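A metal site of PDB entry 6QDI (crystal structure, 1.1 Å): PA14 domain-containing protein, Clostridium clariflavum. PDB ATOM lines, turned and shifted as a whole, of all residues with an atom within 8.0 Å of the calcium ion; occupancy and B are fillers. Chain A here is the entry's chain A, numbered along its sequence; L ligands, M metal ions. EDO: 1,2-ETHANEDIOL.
C of Gly 115 touches the calcium ion, at 3.9 Å.
Six residues have an atom within 4 Å of the calcium ion: Asp 68, Asn 69, Asn 112, Thr 114, Gly 115 and Asn 116.
The guanidinium group (NH2) of Arg 67 sits at hydrogen-bond distance from the backbone carbonyl oxygen (O) of Asn 69.
The side-chain amide nitrogen of Asn 69 lies within hydrogen-bond range of the backbone carbonyl oxygen of Asn 86 (3.0 Å).
The backbone NH of Asn 112 sits at hydrogen-bond distance from the backbone carbonyl oxygen of Tyr 45.
O of Asp 68 sits at hydrogen-bond distance from OH of Tyr 110, at 2.7 Å.
The side-chain carboxylate (OE1) of Glu 43 lies within hydrogen-bond range of the backbone NH (N) of Gly 115 (2.8 Å).
The side-chain amide nitrogen (ND2) of Asn 69 sits at hydrogen-bond distance from the backbone carbonyl oxygen (O) of Leu 87 (3.4 Å).
The side-chain amide oxygen (OD1) of Asn 69 lies close to the backbone NH (N) of Asn 113, 3.0 Å away.
The backbone NH (N) of Thr 114 lies within hydrogen-bond range of the backbone carbonyl oxygen (O) of Glu 43, 2.8 Å away.
The calcium ion is bound by O of Thr 114 (2.3 Å), OD1 of Asp 68 (2.3 Å), OD1 of Asn 112 (2.3 Å), O of Asn 116 (2.4 Å), OD1 of Asn 69 (2.4 Å), O2 of the ligand (2.5 Å) and O1 of the ligand (2.5 Å).
The calcium ion has seven donor atoms within binding distance.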
ATOM      1  N   GLY A  31       5.807 -14.698  -6.663  1.00  0.00           N
ATOM      2  CA  GLY A  31       6.065 -14.046  -7.929  1.00  0.00           C
ATOM      3  C   GLY A  31       7.049 -12.929  -7.675  1.00  0.00           C
ATOM      4  O   GLY A  31       7.941 -13.047  -6.845  1.00  0.00           O
ATOM      5  N   VAL A  32       6.827 -11.829  -8.372  1.00  0.00           N
ATOM      6  CA  VAL A  32       7.676 -10.649  -8.168  1.00  0.00           C
ATOM      7  C   VAL A  32       7.029  -9.653  -7.228  1.00  0.00           C
ATOM      8  O   VAL A  32       7.537  -8.525  -7.106  1.00  0.00           O
ATOM      9  CB  VAL A  32       8.113  -9.962  -9.489  1.00  0.00           C
ATOM     10  CG1 VAL A  32       9.010 -10.898 -10.257  1.00  0.00           C
ATOM     11  CG2 VAL A  32       6.931  -9.517 -10.317  1.00  0.00           C
ATOM     12  N   GLU A  43      11.057  -6.350  -4.232  1.00  0.00           N
ATOM     13  CA  GLU A  43      11.734  -7.609  -4.540  1.00  0.00           C
ATOM     14  C   GLU A  43      12.882  -7.958  -3.610  1.00  0.00           C
ATOM     15  O   GLU A  43      13.621  -8.888  -3.894  1.00  0.00           O
ATOM     16  CB  GLU A  43      12.141  -7.743  -6.017  1.00  0.00           C
ATOM     17  CG  GLU A  43      11.087  -7.319  -7.011  1.00  0.00           C
ATOM     18  CD  GLU A  43      11.536  -7.379  -8.432  1.00  0.00           C
ATOM     19  OE1 GLU A  43      12.576  -8.033  -8.741  1.00  0.00           O
ATOM     20  OE2 GLU A  43      10.848  -6.749  -9.294  1.00  0.00           O
ATOM     21  N   TYR A  45      13.282  -8.931   0.386  1.00  0.00           N
ATOM     22  CA  TYR A  45      12.596  -9.153   1.655  1.00  0.00           C
ATOM     23  C   TYR A  45      13.031 -10.476   2.224  1.00  0.00           C
ATOM     24  O   TYR A  45      13.723 -11.264   1.560  1.00  0.00           O
ATOM     25  CB  TYR A  45      11.040  -9.051   1.486  1.00  0.00           C
ATOM     26  CG  TYR A  45      10.467  -9.991   0.462  1.00  0.00           C
ATOM     27  CD1 TYR A  45      10.183 -11.299   0.784  1.00  0.00           C
ATOM     28  CD2 TYR A  45      10.217  -9.574  -0.847  1.00  0.00           C
ATOM     29  CE1 TYR A  45       9.659 -12.195  -0.175  1.00  0.00           C
ATOM     30  CE2 TYR A  45       9.696 -10.444  -1.787  1.00  0.00           C
ATOM     31  CZ  TYR A  45       9.441 -11.745  -1.442  1.00  0.00           C
ATOM     32  OH  TYR A  45       8.953 -12.659  -2.359  1.00  0.00           O
ATOM     33  N   ARG A  67      13.207 -23.377  -3.077  1.00  0.00           N
ATOM     34  CA  ARG A  67      13.520 -22.036  -2.616  1.00  0.00           C
ATOM     35  C   ARG A  67      13.961 -21.132  -3.763  1.00  0.00           C
ATOM     36  O   ARG A  67      14.738 -21.516  -4.647  1.00  0.00           O
ATOM     37  CB  ARG A  67      14.651 -22.055  -1.574  1.00  0.00           C
ATOM     38  CG  ARG A  67      15.987 -22.575  -2.118  1.00  0.00           C
ATOM     39  CD  ARG A  67      17.082 -22.699  -1.122  1.00  0.00           C
ATOM     40  NE  ARG A  67      18.335 -23.105  -1.742  1.00  0.00           N
ATOM     41  CZ  ARG A  67      19.250 -22.291  -2.242  1.00  0.00           C
ATOM     42  NH1 ARG A  67      20.360 -22.812  -2.726  1.00  0.00           N
ATOM     43  NH2 ARG A  67      19.061 -20.969  -2.238  1.00  0.00           N
ATOM     44  N   ASP A  68      13.564 -19.868  -3.629  1.00  0.00           N
ATOM     45  CA  ASP A  68      14.112 -18.775  -4.442  1.00  0.00           C
ATOM     46  C   ASP A  68      13.947 -17.571  -3.523  1.00  0.00           C
ATOM     47  O   ASP A  68      12.817 -17.117  -3.392  1.00  0.00           O
ATOM     48  CB  ASP A  68      13.357 -18.661  -5.750  1.00  0.00           C
ATOM     49  CG  ASP A  68      13.817 -17.516  -6.570  1.00  0.00           C
ATOM     50  OD1 ASP A  68      14.561 -16.640  -6.056  1.00  0.00           O
ATOM     51  OD2 ASP A  68      13.408 -17.449  -7.783  1.00  0.00           O
ATOM     52  N   ASN A  69      14.961 -17.075  -2.803  1.00  0.00           N
ATOM     53  CA  ASN A  69      16.356 -17.449  -2.871  1.00  0.00           C
ATOM     54  C   ASN A  69      16.817 -18.293  -1.667  1.00  0.00           C
ATOM     55  O   ASN A  69      16.618 -19.505  -1.689  1.00  0.00           O
ATOM     56  CB  ASN A  69      17.230 -16.193  -3.066  1.00  0.00           C
ATOM     57  CG  ASN A  69      16.997 -15.585  -4.421  1.00  0.00           C
ATOM     58  OD1 ASN A  69      16.235 -14.615  -4.566  1.00  0.00           O
ATOM     59  ND2 ASN A  69      17.549 -16.222  -5.446  1.00  0.00           N
ATOM     60  N   GLY A  70      17.419 -17.705  -0.659  1.00  0.00           N
ATOM     61  CA  GLY A  70      18.108 -18.496   0.356  1.00  0.00           C
ATOM     62  C   GLY A  70      17.188 -19.044   1.439  1.00  0.00           C
ATOM     63  O   GLY A  70      16.175 -18.450   1.774  1.00  0.00           O
ATOM     64  N   ASN A  86      22.126 -17.146  -3.333  1.00  0.00           N
ATOM     65  CA  ASN A  86      21.288 -16.582  -4.391  1.00  0.00           C
ATOM     66  C   ASN A  86      20.879 -17.512  -5.470  1.00  0.00           C
ATOM     67  O   ASN A  86      20.234 -17.079  -6.432  1.00  0.00           O
ATOM     68  CB  ASN A  86      21.988 -15.365  -4.977  1.00  0.00           C
ATOM     69  CG  ASN A  86      21.995 -14.238  -3.984  1.00  0.00           C
ATOM     70  OD1 ASN A  86      20.962 -13.729  -3.679  1.00  0.00           O
ATOM     71  ND2 ASN A  86      23.129 -13.927  -3.395  1.00  0.00           N
ATOM     72  N   LEU A  87      21.225 -18.777  -5.358  1.00  0.00           N
ATOM     73  CA  LEU A  87      20.774 -19.718  -6.324  1.00  0.00           C
ATOM     74  C   LEU A  87      19.238 -19.915  -6.117  1.00  0.00           C
ATOM     75  O   LEU A  87      18.562 -19.411  -5.145  1.00  0.00           O
ATOM     76  CB  LEU A  87      21.543 -21.027  -6.168  1.00  0.00           C
ATOM     77  CG  LEU A  87      23.067 -20.935  -6.250  1.00  0.00           C
ATOM     78  CD1 LEU A  87      23.692 -22.288  -5.978  1.00  0.00           C
ATOM     79  CD2 LEU A  87      23.459 -20.409  -7.635  1.00  0.00           C
ATOM     80  N   VAL A  88      18.710 -20.715  -7.018  1.00  0.00           N
ATOM     81  CA  VAL A  88      17.373 -21.295  -6.891  1.00  0.00           C
ATOM     82  C   VAL A  88      17.567 -22.768  -6.628  1.00  0.00           C
ATOM     83  O   VAL A  88      18.278 -23.453  -7.376  1.00  0.00           O
ATOM     84  CB  VAL A  88      16.558 -21.035  -8.144  1.00  0.00           C
ATOM     85  CG1 VAL A  88      15.238 -21.773  -8.085  1.00  0.00           C
ATOM     86  CG2 VAL A  88      16.338 -19.521  -8.320  1.00  0.00           C
ATOM     87  N   TYR A 110      14.448 -17.319   5.456  1.00  0.00           N
ATOM     88  CA  TYR A 110      14.268 -17.262   4.008  1.00  0.00           C
ATOM     89  C   TYR A 110      14.568 -15.844   3.515  1.00  0.00           C
ATOM     90  O   TYR A 110      14.214 -14.869   4.214  1.00  0.00           O
ATOM     91  CB  TYR A 110      12.793 -17.636   3.697  1.00  0.00           C
ATOM     92  CG  TYR A 110      12.383 -17.189   2.310  1.00  0.00           C
ATOM     93  CD1 TYR A 110      12.703 -17.929   1.186  1.00  0.00           C
ATOM     94  CD2 TYR A 110      11.772 -15.956   2.121  1.00  0.00           C
ATOM     95  CE1 TYR A 110      12.411 -17.455  -0.083  1.00  0.00           C
ATOM     96  CE2 TYR A 110      11.526 -15.440   0.865  1.00  0.00           C
ATOM     97  CZ  TYR A 110      11.860 -16.189  -0.244  1.00  0.00           C
ATOM     98  OH  TYR A 110      11.599 -15.679  -1.489  1.00  0.00           O
ATOM     99  N   PHE A 111      15.099 -15.710   2.294  1.00  0.00           N
ATOM    100  CA  PHE A 111      15.147 -14.409   1.651  1.00  0.00           C
ATOM    101  C   PHE A 111      14.873 -14.459   0.184  1.00  0.00           C
ATOM    102  O   PHE A 111      15.204 -15.442  -0.498  1.00  0.00           O
ATOM    103  CB  PHE A 111      16.472 -13.643   1.942  1.00  0.00           C
ATOM    104  CG  PHE A 111      17.699 -14.143   1.207  1.00  0.00           C
ATOM    105  CD1 PHE A 111      18.036 -13.648  -0.057  1.00  0.00           C
ATOM    106  CD2 PHE A 111      18.543 -15.068   1.779  1.00  0.00           C
ATOM    107  CE1 PHE A 111      19.178 -14.057  -0.707  1.00  0.00           C
ATOM    108  CE2 PHE A 111      19.704 -15.466   1.125  1.00  0.00           C
ATOM    109  CZ  PHE A 111      20.032 -14.987  -0.107  1.00  0.00           C
ATOM    110  N   ASN A 112      14.349 -13.343  -0.320  1.00  0.00           N
ATOM    111  CA  ASN A 112      14.271 -13.052  -1.750  1.00  0.00           C
ATOM    112  C   ASN A 112      15.188 -11.888  -2.052  1.00  0.00           C
ATOM    113  O   ASN A 112      15.063 -10.832  -1.441  1.00  0.00           O
ATOM    114  CB  ASN A 112      12.869 -12.742  -2.223  1.00  0.00           C
ATOM    115  CG  ASN A 112      12.781 -12.721  -3.738  1.00  0.00           C
ATOM    116  OD1 ASN A 112      13.635 -13.316  -4.390  1.00  0.00           O
ATOM    117  ND2 ASN A 112      11.784 -12.047  -4.317  1.00  0.00           N
ATOM    118  N   ASN A 113      16.082 -12.061  -3.031  1.00  0.00           N
ATOM    119  CA  ASN A 113      16.996 -11.018  -3.478  1.00  0.00           C
ATOM    120  C   ASN A 113      16.780 -10.805  -4.989  1.00  0.00           C
ATOM    121  O   ASN A 113      17.599 -11.252  -5.796  1.00  0.00           O
ATOM    122  CB  ASN A 113      18.426 -11.414  -3.180  1.00  0.00           C
ATOM    123  CG  ASN A 113      19.431 -10.339  -3.543  1.00  0.00           C
ATOM    124  OD1 ASN A 113      19.118  -9.221  -3.851  1.00  0.00           O
ATOM    125  ND2 ASN A 113      20.665 -10.705  -3.476  1.00  0.00           N
ATOM    126  N   THR A 114      15.693 -10.107  -5.297  1.00  0.00           N
ATOM    127  CA  THR A 114      15.175  -9.780  -6.658  1.00  0.00           C
ATOM    128  C   THR A 114      14.471 -10.955  -7.308  1.00  0.00           C
ATOM    129  O   THR A 114      14.692 -12.141  -6.998  1.00  0.00           O
ATOM    130  CB  THR A 114      16.220  -9.202  -7.628  1.00  0.00           C
ATOM    131  OG1 THR A 114      17.081 -10.220  -8.170  1.00  0.00           O
ATOM    132  CG2 THR A 114      17.022  -8.091  -6.981  1.00  0.00           C
ATOM    133  N   GLY A 115      13.606 -10.613  -8.261  1.00  0.00           N
ATOM    134  CA  GLY A 115      12.920 -11.596  -9.058  1.00  0.00           C
ATOM    135  C   GLY A 115      11.877 -12.351  -8.270  1.00  0.00           C
ATOM    136  O   GLY A 115      11.349 -11.890  -7.258  1.00  0.00           O
ATOM    137  N   ASN A 116      11.561 -13.532  -8.784  1.00  0.00           N
ATOM    138  CA  ASN A 116      10.588 -14.405  -8.163  1.00  0.00           C
ATOM    139  C   ASN A 116      11.025 -14.712  -6.728  1.00  0.00           C
ATOM    140  O   ASN A 116      12.220 -14.817  -6.421  1.00  0.00           O
ATOM    141  CB  ASN A 116      10.513 -15.717  -8.951  1.00  0.00           C
ATOM    142  CG  ASN A 116       9.176 -16.466  -8.763  1.00  0.00           C
ATOM    143  OD1 ASN A 116       8.313 -16.098  -7.966  1.00  0.00           O
ATOM    144  ND2 ASN A 116       9.040 -17.561  -9.515  1.00  0.00           N
ATOM    145  N   GLY A 117      10.036 -14.944  -5.871  1.00  0.00           N
ATOM    146  CA  GLY A 117      10.248 -15.422  -4.521  1.00  0.00           C
ATOM    147  C   GLY A 117       9.287 -16.574  -4.238  1.00  0.00           C
ATOM    148  O   GLY A 117       8.105 -16.438  -4.479  1.00  0.00           O
ATOM    149  N   PHE A 118       9.834 -17.686  -3.734  1.00  0.00           N
ATOM    150  CA  PHE A 118       9.012 -18.812  -3.341  1.00  0.00           C
ATOM    151  C   PHE A 118       9.764 -19.631  -2.289  1.00  0.00           C
ATOM    152  O   PHE A 118      10.991 -19.662  -2.270  1.00  0.00           O
ATOM    153  CB  PHE A 118       8.538 -19.668  -4.524  1.00  0.00           C
ATOM    154  CG  PHE A 118       9.617 -20.171  -5.441  1.00  0.00           C
ATOM    155  CD1 PHE A 118      10.411 -21.260  -5.082  1.00  0.00           C
ATOM    156  CD2 PHE A 118       9.743 -19.649  -6.716  1.00  0.00           C
ATOM    157  CE1 PHE A 118      11.363 -21.771  -5.963  1.00  0.00           C
ATOM    158  CE2 PHE A 118      10.677 -20.181  -7.614  1.00  0.00           C
ATOM    159  CZ  PHE A 118      11.478 -21.214  -7.236  1.00  0.00           C
HETATM  160  C1  EDO L   1      15.476 -15.282  -9.344  1.00  0.00           C
HETATM  161  O1  EDO L   1      14.234 -15.061  -8.654  1.00  0.00           O
HETATM  162  C2  EDO L   1      16.492 -14.210  -8.912  1.00  0.00           C
HETATM  163  O2  EDO L   1      16.657 -14.385  -7.538  1.00  0.00           O
HETATM  164 CA    CA M   1      14.534 -14.334  -6.304  1.00  0.00          CA
